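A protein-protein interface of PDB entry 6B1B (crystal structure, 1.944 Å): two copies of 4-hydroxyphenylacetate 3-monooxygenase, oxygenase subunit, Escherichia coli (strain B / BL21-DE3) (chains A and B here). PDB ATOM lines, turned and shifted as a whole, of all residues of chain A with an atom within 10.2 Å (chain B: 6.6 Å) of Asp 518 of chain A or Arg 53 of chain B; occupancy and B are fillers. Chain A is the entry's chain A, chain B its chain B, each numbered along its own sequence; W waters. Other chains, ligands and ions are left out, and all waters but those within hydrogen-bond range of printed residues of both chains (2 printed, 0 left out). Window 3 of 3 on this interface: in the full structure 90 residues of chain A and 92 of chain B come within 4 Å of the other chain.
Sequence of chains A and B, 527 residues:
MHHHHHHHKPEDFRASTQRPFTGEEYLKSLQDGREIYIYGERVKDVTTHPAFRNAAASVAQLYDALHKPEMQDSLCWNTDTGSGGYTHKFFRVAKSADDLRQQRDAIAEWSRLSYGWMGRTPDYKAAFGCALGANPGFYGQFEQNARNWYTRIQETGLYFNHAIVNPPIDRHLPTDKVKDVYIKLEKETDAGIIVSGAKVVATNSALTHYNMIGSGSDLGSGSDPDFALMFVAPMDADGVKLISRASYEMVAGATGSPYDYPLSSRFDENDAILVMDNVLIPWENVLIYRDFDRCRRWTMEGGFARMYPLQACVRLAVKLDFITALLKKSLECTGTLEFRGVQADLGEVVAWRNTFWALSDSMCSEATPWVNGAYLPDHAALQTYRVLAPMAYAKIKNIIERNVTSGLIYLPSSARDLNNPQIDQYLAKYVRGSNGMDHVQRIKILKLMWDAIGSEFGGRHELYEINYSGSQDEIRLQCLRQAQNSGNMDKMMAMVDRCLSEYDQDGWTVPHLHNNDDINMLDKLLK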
ATOM      1  N   TRP A 508      30.546 -10.320   4.725  1.00  0.00           N
ATOM      2  CA  TRP A 508      31.148 -10.524   3.411  1.00  0.00           C
ATOM      3  C   TRP A 508      32.070  -9.363   3.056  1.00  0.00           C
ATOM      4  O   TRP A 508      31.853  -8.225   3.465  1.00  0.00           O
ATOM      5  CB  TRP A 508      30.077 -10.638   2.326  1.00  0.00           C
ATOM      6  CG  TRP A 508      29.097 -11.753   2.519  1.00  0.00           C
ATOM      7  CD1 TRP A 508      27.756 -11.633   2.757  1.00  0.00           C
ATOM      8  CD2 TRP A 508      29.374 -13.158   2.472  1.00  0.00           C
ATOM      9  NE1 TRP A 508      27.184 -12.880   2.865  1.00  0.00           N
ATOM     10  CE2 TRP A 508      28.154 -13.830   2.686  1.00  0.00           C
ATOM     11  CE3 TRP A 508      30.534 -13.911   2.260  1.00  0.00           C
ATOM     12  CZ2 TRP A 508      28.062 -15.217   2.717  1.00  0.00           C
ATOM     13  CZ3 TRP A 508      30.442 -15.288   2.290  1.00  0.00           C
ATOM     14  CH2 TRP A 508      29.207 -15.928   2.512  1.00  0.00           C
ATOM     15  N   PRO A 511      30.800  -7.837  -3.055  1.00  0.00           N
ATOM     16  CA  PRO A 511      29.495  -7.161  -3.153  1.00  0.00           C
ATOM     17  C   PRO A 511      28.329  -8.052  -3.556  1.00  0.00           C
ATOM     18  O   PRO A 511      27.179  -7.652  -3.336  1.00  0.00           O
ATOM     19  CB  PRO A 511      29.741  -6.087  -4.230  1.00  0.00           C
ATOM     20  CG  PRO A 511      30.799  -6.682  -5.095  1.00  0.00           C
ATOM     21  CD  PRO A 511      31.719  -7.413  -4.127  1.00  0.00           C
ATOM     22  N   HIS A 512      28.560  -9.229  -4.146  1.00  0.00           N
ATOM     23  CA  HIS A 512      27.435  -9.940  -4.748  1.00  0.00           C
ATOM     24  C   HIS A 512      26.604 -10.740  -3.746  1.00  0.00           C
ATOM     25  O   HIS A 512      25.501 -11.183  -4.097  1.00  0.00           O
ATOM     26  CB  HIS A 512      27.919 -10.854  -5.876  1.00  0.00           C
ATOM     27  CG  HIS A 512      28.629 -12.089  -5.412  1.00  0.00           C
ATOM     28  ND1 HIS A 512      29.944 -12.081  -4.999  1.00  0.00           N
ATOM     29  CD2 HIS A 512      28.221 -13.378  -5.340  1.00  0.00           C
ATOM     30  CE1 HIS A 512      30.310 -13.310  -4.674  1.00  0.00           C
ATOM     31  NE2 HIS A 512      29.284 -14.117  -4.874  1.00  0.00           N
ATOM     32  N   LEU A 513      27.082 -10.928  -2.521  1.00  0.00           N
ATOM     33  CA  LEU A 513      26.354 -11.713  -1.532  1.00  0.00           C
ATOM     34  C   LEU A 513      25.629 -10.794  -0.554  1.00  0.00           C
ATOM     35  O   LEU A 513      26.006  -9.637  -0.354  1.00  0.00           O
ATOM     36  CB  LEU A 513      27.303 -12.653  -0.785  1.00  0.00           C
ATOM     37  CG  LEU A 513      27.941 -13.696  -1.720  1.00  0.00           C
ATOM     38  CD1 LEU A 513      29.174 -14.347  -1.061  1.00  0.00           C
ATOM     39  CD2 LEU A 513      26.893 -14.757  -2.137  1.00  0.00           C
ATOM     40  N   HIS A 514      24.562 -11.321   0.043  1.00  0.00           N
ATOM     41  CA  HIS A 514      23.704 -10.540   0.931  1.00  0.00           C
ATOM     42  C   HIS A 514      24.237 -10.542   2.357  1.00  0.00           C
ATOM     43  O   HIS A 514      24.554 -11.597   2.909  1.00  0.00           O
ATOM     44  CB  HIS A 514      22.282 -11.088   0.942  1.00  0.00           C
ATOM     45  CG  HIS A 514      21.595 -11.008  -0.380  1.00  0.00           C
ATOM     46  ND1 HIS A 514      20.695 -10.013  -0.695  1.00  0.00           N
ATOM     47  CD2 HIS A 514      21.678 -11.802  -1.472  1.00  0.00           C
ATOM     48  CE1 HIS A 514      20.246 -10.203  -1.924  1.00  0.00           C
ATOM     49  NE2 HIS A 514      20.831 -11.279  -2.419  1.00  0.00           N
ATOM     50  N   ASN A 515      24.343  -9.349   2.933  1.00  0.00           N
ATOM     51  CA  ASN A 515      24.493  -9.173   4.370  1.00  0.00           C
ATOM     52  C   ASN A 515      23.365  -9.887   5.113  1.00  0.00           C
ATOM     53  O   ASN A 515      22.198  -9.767   4.741  1.00  0.00           O
ATOM     54  CB  ASN A 515      24.469  -7.665   4.657  1.00  0.00           C
ATOM     55  CG  ASN A 515      24.967  -7.306   6.033  1.00  0.00           C
ATOM     56  OD1 ASN A 515      24.737  -8.028   7.000  1.00  0.00           O
ATOM     57  ND2 ASN A 515      25.642  -6.159   6.131  1.00  0.00           N
ATOM     58  N   ASN A 516      23.699 -10.644   6.160  1.00  0.00           N
ATOM     59  CA  ASN A 516      22.654 -11.325   6.928  1.00  0.00           C
ATOM     60  C   ASN A 516      22.103 -10.468   8.074  1.00  0.00           C
ATOM     61  O   ASN A 516      21.285 -10.958   8.858  1.00  0.00           O
ATOM     62  CB  ASN A 516      23.150 -12.673   7.481  1.00  0.00           C
ATOM     63  CG  ASN A 516      24.150 -12.526   8.618  1.00  0.00           C
ATOM     64  OD1 ASN A 516      24.971 -11.609   8.630  1.00  0.00           O
ATOM     65  ND2 ASN A 516      24.079 -13.437   9.589  1.00  0.00           N
ATOM     66  N   ASP A 517      22.503  -9.196   8.174  1.00  0.00           N
ATOM     67  CA  ASP A 517      22.005  -8.363   9.272  1.00  0.00           C
ATOM     68  C   ASP A 517      20.488  -8.251   9.254  1.00  0.00           C
ATOM     69  O   ASP A 517      19.862  -8.154  10.315  1.00  0.00           O
ATOM     70  CB  ASP A 517      22.637  -6.971   9.221  1.00  0.00           C
ATOM     71  CG  ASP A 517      24.088  -6.982   9.649  1.00  0.00           C
ATOM     72  OD1 ASP A 517      24.588  -8.061  10.031  1.00  0.00           O
ATOM     73  OD2 ASP A 517      24.734  -5.917   9.587  1.00  0.00           O
ATOM     74  N   ASP A 518      19.875  -8.297   8.068  1.00  0.00           N
ATOM     75  CA  ASP A 518      18.427  -8.169   7.975  1.00  0.00           C
ATOM     76  C   ASP A 518      17.694  -9.421   8.429  1.00  0.00           C
ATOM     77  O   ASP A 518      16.482  -9.354   8.659  1.00  0.00           O
ATOM     78  CB  ASP A 518      18.003  -7.826   6.542  1.00  0.00           C
ATOM     79  CG  ASP A 518      18.585  -8.778   5.503  1.00  0.00           C
ATOM     80  OD1 ASP A 518      19.364  -9.686   5.870  1.00  0.00           O
ATOM     81  OD2 ASP A 518      18.252  -8.629   4.308  1.00  0.00           O
ATOM     82  N   ILE A 519      18.377 -10.560   8.552  1.00  0.00           N
ATOM     83  CA  ILE A 519      17.723 -11.804   8.945  1.00  0.00           C
ATOM     84  C   ILE A 519      18.312 -12.407  10.206  1.00  0.00           C
ATOM     85  O   ILE A 519      17.802 -13.426  10.685  1.00  0.00           O
ATOM     86  CB  ILE A 519      17.740 -12.851   7.807  1.00  0.00           C
ATOM     87  CG1 ILE A 519      19.177 -13.215   7.411  1.00  0.00           C
ATOM     88  CG2 ILE A 519      16.938 -12.358   6.581  1.00  0.00           C
ATOM     89  CD1 ILE A 519      19.268 -14.441   6.490  1.00  0.00           C
ATOM     90  N   ASN A 520      19.368 -11.820  10.761  1.00  0.00           N
ATOM     91  CA  ASN A 520      20.001 -12.406  11.931  1.00  0.00           C
ATOM     92  C   ASN A 520      19.136 -12.183  13.167  1.00  0.00           C
ATOM     93  O   ASN A 520      18.757 -11.053  13.477  1.00  0.00           O
ATOM     94  CB  ASN A 520      21.389 -11.817  12.148  1.00  0.00           C
ATOM     95  CG  ASN A 520      22.189 -12.624  13.142  1.00  0.00           C
ATOM     96  OD1 ASN A 520      22.081 -12.421  14.347  1.00  0.00           O
ATOM     97  ND2 ASN A 520      22.949 -13.597  12.643  1.00  0.00           N
ATOM     98  N   MET A 521      18.837 -13.269  13.873  1.00  0.00           N
ATOM     99  CA  MET A 521      17.896 -13.266  14.982  1.00  0.00           C
ATOM    100  C   MET A 521      18.579 -13.343  16.344  1.00  0.00           C
ATOM    101  O   MET A 521      17.890 -13.465  17.364  1.00  0.00           O
ATOM    102  CB  MET A 521      16.916 -14.438  14.828  1.00  0.00           C
ATOM    103  CG  MET A 521      16.064 -14.381  13.564  1.00  0.00           C
ATOM    104  SD  MET A 521      14.901 -12.987  13.648  1.00  0.00           S
ATOM    105  CE  MET A 521      14.610 -12.628  11.918  1.00  0.00           C
ATOM    106  N   LEU A 522      19.912 -13.268  16.396  1.00  0.00           N
ATOM    107  CA  LEU A 522      20.600 -13.569  17.653  1.00  0.00           C
ATOM    108  C   LEU A 522      20.344 -12.494  18.707  1.00  0.00           C
ATOM    109  O   LEU A 522      20.185 -12.809  19.894  1.00  0.00           O
ATOM    110  CB  LEU A 522      22.099 -13.740  17.403  1.00  0.00           C
ATOM    111  CG  LEU A 522      22.488 -14.970  16.556  1.00  0.00           C
ATOM    112  CD1 LEU A 522      23.972 -14.975  16.235  1.00  0.00           C
ATOM    113  CD2 LEU A 522      22.092 -16.268  17.254  1.00  0.00           C
ATOM    114  N   ASP A 523      20.283 -11.225  18.296  1.00  0.00           N
ATOM    115  CA  ASP A 523      19.953 -10.162  19.247  1.00  0.00           C
ATOM    116  C   ASP A 523      18.595 -10.410  19.890  1.00  0.00           C
ATOM    117  O   ASP A 523      18.444 -10.322  21.114  1.00  0.00           O
ATOM    118  CB  ASP A 523      19.961  -8.805  18.543  1.00  0.00           C
ATOM    119  CG  ASP A 523      21.351  -8.248  18.356  1.00  0.00           C
ATOM    120  OD1 ASP A 523      22.317  -8.810  18.910  1.00  0.00           O
ATOM    121  OD2 ASP A 523      21.475  -7.237  17.631  1.00  0.00           O
ATOM    122  N   LYS A 524      17.583 -10.697  19.067  1.00  0.00           N
ATOM    123  CA  LYS A 524      16.255 -11.006  19.588  1.00  0.00           C
ATOM    124  C   LYS A 524      16.301 -12.185  20.552  1.00  0.00           C
ATOM    125  O   LYS A 524      15.634 -12.175  21.594  1.00  0.00           O
ATOM    126  CB  LYS A 524      15.299 -11.288  18.432  1.00  0.00           C
ATOM    127  CG  LYS A 524      15.062 -10.072  17.555  1.00  0.00           C
ATOM    128  CD  LYS A 524      13.980 -10.315  16.518  1.00  0.00           C
ATOM    129  CE  LYS A 524      13.516  -9.011  15.880  1.00  0.00           C
ATOM    130  NZ  LYS A 524      13.093  -8.000  16.878  1.00  0.00           N
ATOM    131  N   LEU B  27      19.108 -13.489 -12.583  1.00  0.00           N
ATOM    132  CA  LEU B  27      18.336 -13.257 -11.365  1.00  0.00           C
ATOM    133  C   LEU B  27      16.954 -12.698 -11.685  1.00  0.00           C
ATOM    134  O   LEU B  27      15.951 -13.152 -11.122  1.00  0.00           O
ATOM    135  CB  LEU B  27      19.105 -12.333 -10.421  1.00  0.00           C
ATOM    136  CG  LEU B  27      20.387 -12.982  -9.887  1.00  0.00           C
ATOM    137  CD1 LEU B  27      21.304 -11.947  -9.223  1.00  0.00           C
ATOM    138  CD2 LEU B  27      20.064 -14.133  -8.933  1.00  0.00           C
ATOM    139  N   ASP B  45       9.891 -14.695  -3.673  1.00  0.00           N
ATOM    140  CA  ASP B  45      10.888 -14.383  -4.700  1.00  0.00           C
ATOM    141  C   ASP B  45      12.192 -15.061  -4.287  1.00  0.00           C
ATOM    142  O   ASP B  45      12.801 -14.638  -3.301  1.00  0.00           O
ATOM    143  CB  ASP B  45      11.052 -12.865  -4.807  1.00  0.00           C
ATOM    144  CG  ASP B  45      12.040 -12.421  -5.879  1.00  0.00           C
ATOM    145  OD1 ASP B  45      12.858 -13.234  -6.373  1.00  0.00           O
ATOM    146  OD2 ASP B  45      12.005 -11.208  -6.215  1.00  0.00           O
ATOM    147  N   VAL B  46      12.636 -16.081  -5.044  1.00  0.00           N
ATOM    148  CA  VAL B  46      13.841 -16.820  -4.635  1.00  0.00           C
ATOM    149  C   VAL B  46      15.064 -15.921  -4.610  1.00  0.00           C
ATOM    150  O   VAL B  46      16.011 -16.188  -3.863  1.00  0.00           O
ATOM    151  CB  VAL B  46      14.122 -18.047  -5.534  1.00  0.00           C
ATOM    152  CG1 VAL B  46      13.088 -19.107  -5.344  1.00  0.00           C
ATOM    153  CG2 VAL B  46      14.253 -17.642  -7.021  1.00  0.00           C
ATOM    154  N   THR B  47      15.086 -14.849  -5.413  1.00  0.00           N
ATOM    155  CA  THR B  47      16.290 -14.018  -5.423  1.00  0.00           C
ATOM    156  C   THR B  47      16.406 -13.116  -4.202  1.00  0.00           C
ATOM    157  O   THR B  47      17.478 -12.535  -3.986  1.00  0.00           O
ATOM    158  CB  THR B  47      16.367 -13.143  -6.687  1.00  0.00           C
ATOM    159  OG1 THR B  47      15.365 -12.113  -6.638  1.00  0.00           O
ATOM    160  CG2 THR B  47      16.173 -13.993  -7.933  1.00  0.00           C
ATOM    161  N   THR B  48      15.347 -12.969  -3.409  1.00  0.00           N
ATOM    162  CA  THR B  48      15.410 -12.175  -2.189  1.00  0.00           C
ATOM    163  C   THR B  48      15.086 -12.976  -0.939  1.00  0.00           C
ATOM    164  O   THR B  48      15.257 -12.457   0.170  1.00  0.00           O
ATOM    165  CB  THR B  48      14.442 -10.978  -2.258  1.00  0.00           C
ATOM    166  OG1 THR B  48      13.091 -11.457  -2.307  1.00  0.00           O
ATOM    167  CG2 THR B  48      14.709 -10.139  -3.498  1.00  0.00           C
ATOM    168  N   HIS B  49      14.627 -14.212  -1.085  1.00  0.00           N
ATOM    169  CA  HIS B  49      14.192 -14.994   0.059  1.00  0.00           C
ATOM    170  C   HIS B  49      15.386 -15.418   0.920  1.00  0.00           C
ATOM    171  O   HIS B  49      16.445 -15.768   0.391  1.00  0.00           O
ATOM    172  CB  HIS B  49      13.410 -16.213  -0.424  1.00  0.00           C
ATOM    173  CG  HIS B  49      12.678 -16.919   0.670  1.00  0.00           C
ATOM    174  ND1 HIS B  49      13.278 -17.864   1.471  1.00  0.00           N
ATOM    175  CD2 HIS B  49      11.409 -16.789   1.123  1.00  0.00           C
ATOM    176  CE1 HIS B  49      12.403 -18.306   2.355  1.00  0.00           C
ATOM    177  NE2 HIS B  49      11.262 -17.666   2.168  1.00  0.00           N
ATOM    178  N   PRO B  50      15.243 -15.403   2.252  1.00  0.00           N
ATOM    179  CA  PRO B  50      16.385 -15.745   3.129  1.00  0.00           C
ATOM    180  C   PRO B  50      16.928 -17.158   2.926  1.00  0.00           C
ATOM    181  O   PRO B  50      18.071 -17.426   3.313  1.00  0.00           O
ATOM    182  CB  PRO B  50      15.813 -15.589   4.546  1.00  0.00           C
ATOM    183  CG  PRO B  50      14.565 -14.790   4.402  1.00  0.00           C
ATOM    184  CD  PRO B  50      14.060 -14.935   3.003  1.00  0.00           C
ATOM    185  N   ALA B  51      16.153 -18.068   2.352  1.00  0.00           N
ATOM    186  CA  ALA B  51      16.614 -19.437   2.157  1.00  0.00           C
ATOM    187  C   ALA B  51      17.348 -19.655   0.839  1.00  0.00           C
ATOM    188  O   ALA B  51      18.006 -20.689   0.683  1.00  0.00           O
ATOM    189  CB  ALA B  51      15.427 -20.399   2.228  1.00  0.00           C
ATOM    190  N   PHE B  52      17.252 -18.719  -0.113  1.00  0.00           N
ATOM    191  CA  PHE B  52      17.730 -18.953  -1.472  1.00  0.00           C
ATOM    192  C   PHE B  52      18.569 -17.827  -2.062  1.00  0.00           C
ATOM    193  O   PHE B  52      19.253 -18.065  -3.067  1.00  0.00           O
ATOM    194  CB  PHE B  52      16.539 -19.201  -2.419  1.00  0.00           C
ATOM    195  CG  PHE B  52      15.711 -20.403  -2.061  1.00  0.00           C
ATOM    196  CD1 PHE B  52      16.106 -21.676  -2.452  1.00  0.00           C
ATOM    197  CD2 PHE B  52      14.532 -20.263  -1.335  1.00  0.00           C
ATOM    198  CE1 PHE B  52      15.347 -22.788  -2.118  1.00  0.00           C
ATOM    199  CE2 PHE B  52      13.769 -21.371  -1.000  1.00  0.00           C
ATOM    200  CZ  PHE B  52      14.171 -22.633  -1.392  1.00  0.00           C
ATOM    201  N   ARG B  53      18.549 -16.620  -1.484  1.00  0.00           N
ATOM    202  CA  ARG B  53      19.067 -15.446  -2.182  1.00  0.00           C
ATOM    203  C   ARG B  53      20.572 -15.539  -2.441  1.00  0.00           C
ATOM    204  O   ARG B  53      21.059 -15.065  -3.478  1.00  0.00           O
ATOM    205  CB  ARG B  53      18.736 -14.184  -1.376  1.00  0.00           C
ATOM    206  CG  ARG B  53      19.368 -14.161   0.010  1.00  0.00           C
ATOM    207  CD  ARG B  53      18.751 -13.073   0.886  1.00  0.00           C
ATOM    208  NE  ARG B  53      19.467 -12.971   2.157  1.00  0.00           N
ATOM    209  CZ  ARG B  53      19.395 -11.923   2.974  1.00  0.00           C
ATOM    210  NH1 ARG B  53      18.630 -10.895   2.647  1.00  0.00           N
ATOM    211  NH2 ARG B  53      20.084 -11.902   4.110  1.00  0.00           N
ATOM    212  N   ASN B  54      21.335 -16.131  -1.513  1.00  0.00           N
ATOM    213  CA  ASN B  54      22.778 -16.182  -1.732  1.00  0.00           C
ATOM    214  C   ASN B  54      23.154 -17.290  -2.707  1.00  0.00           C
ATOM    215  O   ASN B  54      24.049 -17.104  -3.541  1.00  0.00           O
ATOM    216  CB  ASN B  54      23.525 -16.368  -0.407  1.00  0.00           C
ATOM    217  CG  ASN B  54      23.592 -15.085   0.410  1.00  0.00           C
ATOM    218  OD1 ASN B  54      23.510 -13.982  -0.149  1.00  0.00           O
ATOM    219  ND2 ASN B  54      23.731 -15.219   1.733  1.00  0.00           N
ATOM    220  N   ALA B  55      22.490 -18.445  -2.613  1.00  0.00           N
ATOM    221  CA  ALA B  55      22.716 -19.494  -3.604  1.00  0.00           C
ATOM    222  C   ALA B  55      22.407 -18.980  -5.004  1.00  0.00           C
ATOM    223  O   ALA B  55      23.159 -19.249  -5.947  1.00  0.00           O
ATOM    224  CB  ALA B  55      21.875 -20.730  -3.272  1.00  0.00           C
ATOM    225  N   ALA B  56      21.321 -18.215  -5.154  1.00  0.00           N
ATOM    226  CA  ALA B  56      21.007 -17.606  -6.445  1.00  0.00           C
ATOM    227  C   ALA B  56      22.123 -16.668  -6.892  1.00  0.00           C
ATOM    228  O   ALA B  56      22.559 -16.702  -8.052  1.00  0.00           O
ATOM    229  CB  ALA B  56      19.682 -16.843  -6.360  1.00  0.00           C
ATOM    230  N   ALA B  57      22.605 -15.829  -5.973  1.00  0.00           N
ATOM    231  CA  ALA B  57      23.717 -14.933  -6.282  1.00  0.00           C
ATOM    232  C   ALA B  57      24.971 -15.705  -6.675  1.00  0.00           C
ATOM    233  O   ALA B  57      25.746 -15.256  -7.527  1.00  0.00           O
ATOM    234  CB  ALA B  57      24.010 -14.035  -5.076  1.00  0.00           C
ATOM    235  N   SER B  58      25.210 -16.847  -6.036  1.00  0.00           N
ATOM    236  CA  SER B  58      26.362 -17.672  -6.389  1.00  0.00           C
ATOM    237  C   SER B  58      26.240 -18.208  -7.814  1.00  0.00           C
ATOM    238  O   SER B  58      27.229 -18.262  -8.552  1.00  0.00           O
ATOM    239  CB  SER B  58      26.495 -18.805  -5.375  1.00  0.00           C
ATOM    240  OG  SER B  58      26.992 -18.281  -4.149  1.00  0.00           O
ATOM    241  N   LEU B 207      16.151 -22.795  -8.258  1.00  0.00           N
ATOM    242  CA  LEU B 207      16.894 -21.771  -8.974  1.00  0.00           C
ATOM    243  C   LEU B 207      16.985 -22.042 -10.470  1.00  0.00           C
ATOM    244  O   LEU B 207      17.755 -21.372 -11.158  1.00  0.00           O
ATOM    245  CB  LEU B 207      18.290 -21.645  -8.364  1.00  0.00           C
ATOM    246  CG  LEU B 207      18.275 -21.364  -6.859  1.00  0.00           C
ATOM    247  CD1 LEU B 207      19.701 -21.225  -6.315  1.00  0.00           C
ATOM    248  CD2 LEU B 207      17.444 -20.117  -6.564  1.00  0.00           C
ATOM    249  N   GLU B 249      21.319 -22.413   4.256  1.00  0.00           N
ATOM    250  CA  GLU B 249      21.567 -20.989   4.033  1.00  0.00           C
ATOM    251  C   GLU B 249      20.776 -20.126   5.013  1.00  0.00           C
ATOM    252  O   GLU B 249      21.330 -19.215   5.640  1.00  0.00           O
ATOM    253  CB  GLU B 249      21.217 -20.594   2.595  1.00  0.00           C
ATOM    254  CG  GLU B 249      21.282 -19.072   2.413  1.00  0.00           C
ATOM    255  CD  GLU B 249      21.087 -18.581   0.972  1.00  0.00           C
ATOM    256  OE1 GLU B 249      21.313 -19.363   0.014  1.00  0.00           O
ATOM    257  OE2 GLU B 249      20.723 -17.390   0.808  1.00  0.00           O
ATOM    258  N   GLY B 253      22.198 -17.834   8.058  1.00  0.00           N
ATOM    259  CA  GLY B 253      21.929 -16.405   8.104  1.00  0.00           C
ATOM    260  C   GLY B 253      21.238 -15.973   9.388  1.00  0.00           C
ATOM    261  O   GLY B 253      21.578 -14.937   9.963  1.00  0.00           O
HETATM  262  O   HOH W   1      19.952 -13.060  -4.984  1.00  0.00           O
HETATM  263  O   HOH W   2      29.305 -17.040  -4.481  1.00  0.00           O
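ND2 of Asn 516 of chain A sits close to ND2 of Asn 520 of chain A. The side-chain hydroxyl of Thr 47 of chain B is in hydrogen-bond range of the side-chain carboxylate of Asp 45 of chain B, at 2.8 Å. The backbone NH (N) of Asn 54 of chain B is in hydrogen-bond range of the side-chain carboxylate (OE2) of Glu 249 of chain B, 2.7 Å away. OG of Ser 58 of chain B sits at hydrogen-bond distance from O of Asn 54 of chain B, at 3.2 Å. The side-chain amide oxygen (OD1) of Asn 515 of chain A lies within hydrogen-bond range of the backbone NH (N) of Asp 517 of chain A, 2.8 Å away. NE1 of Trp 508 of chain A sits at hydrogen-bond distance from O of His 514 of chain A (2.9 Å).
Water W2 lies within hydrogen-bond range of the side-chain hydroxyl of Ser 58 of chain B (2.6 Å) and a ring nitrogen (NE2) of His 512 of chain A (2.9 Å). Water W1 lies within hydrogen-bond range of O of Thr 47 of chain B, O of Arg 53 of chain B and NE2 of His 514 of chain A.
Of the 18 printed residues of chain B, 6 touch a printed residue of chain A. Hydrophobic or aromatic side chains of chain A within 4 Å of the printed part of chain B: His 512, Leu 513, His 514 and Ile 519. Among the printed residues, 13 pairs touch across the chains. Among the printed residues, Asp or Glu carboxylates within 4 Å of a Lys or Arg side-chain nitrogen of the other chain: Asp 518 of chain A with Arg 53 of chain B (2.8 Å).
The backbone carbonyl oxygen (O) of Gly 253 of chain B sits at hydrogen-bond distance from the side-chain amide nitrogen (ND2) of Asn 516 of chain A (2.9 Å). N of His 514 of chain A lies within hydrogen-bond range of OD1 of Asn 54 of chain B (2.9 Å). The backbone carbonyl oxygen of Gly 253 of chain B sits at hydrogen-bond distance from the side-chain amide nitrogen of Asn 520 of chain A (3.3 Å). OD2 of Asp 518 of chain A lies within salt-bridge range of NH1 of Arg 53 of chain B, at 2.8 Å. The guanidinium group (NH2) of Arg 53 of chain B is in hydrogen-bond range of the backbone carbonyl oxygen (O) of Asn 515 of chain A (3.1 Å).
Of the printed residues of chain B, Leu 513 of chain A touches Asn 54. Printed residues of chain B within 4 Å of His 514 of chain A: Thr 47, Arg 53 and Asn 54. Printed residues of chain B within 4 Å of Asn 515 of chain A: Arg 53 (3.1 Å). Of chain B, only Arg 53 (2.8 Å) comes within 4 Å of Asp 518 of chain A. Of the printed residues of chain B, Ile 519 of chain A touches Pro 50 (3.98 Å), Arg 53 (3.6 Å) and Gly 253 (3.7 Å). Asp 523 of chain A touches none of the printed residues of chain B. His 49 of chain B touches none of the printed residues of chain A. Of chain A, only His 514, Asn 515, Asn 516, Asp 518 and Ile 519 come within 4 Å of Arg 53 of chain B. Asn 54 of chain B touches just these residues of chain A: Leu 513 (3.8 Å) and His 514 (2.9 Å). No residue of chain A comes within 4 Å of Ala 55 of chain B. No residue of chain A comes within 4 Å of Ala 56 of chain B. The nearest residue of chain B that does not touch Asp 518 of chain A is Thr 48 of chain B (6.4 Å). The nearest printed residue of chain B that does not touch His 512 of chain A is Ser 58 of chain B (4.6 Å).
No position is printed for both chains. Of the 13 pairs that touch across the chains among the printed residues, none has its exchanged pair printed and touching as well.
Among the printed residues, pairs that only touch across the chains: His 512 of chain A with Ala 57 of chain B (3.4 Å), Ile 519 of chain A with Arg 53 of chain B (3.6 Å), His 514 of chain A with Arg 53 of chain B (3.6 Å), Ile 519 of chain A with Gly 253 of chain B (3.7 Å), Leu 513 of chain A with Asn 54 of chain B (3.8 Å), Asn 516 of chain A with Arg 53 of chain B (3.9 Å), His 514 of chain A with Thr 47 of chain B (3.9 Å) and Ile 519 of chain A with Pro 50 of chain B (3.98 Å).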
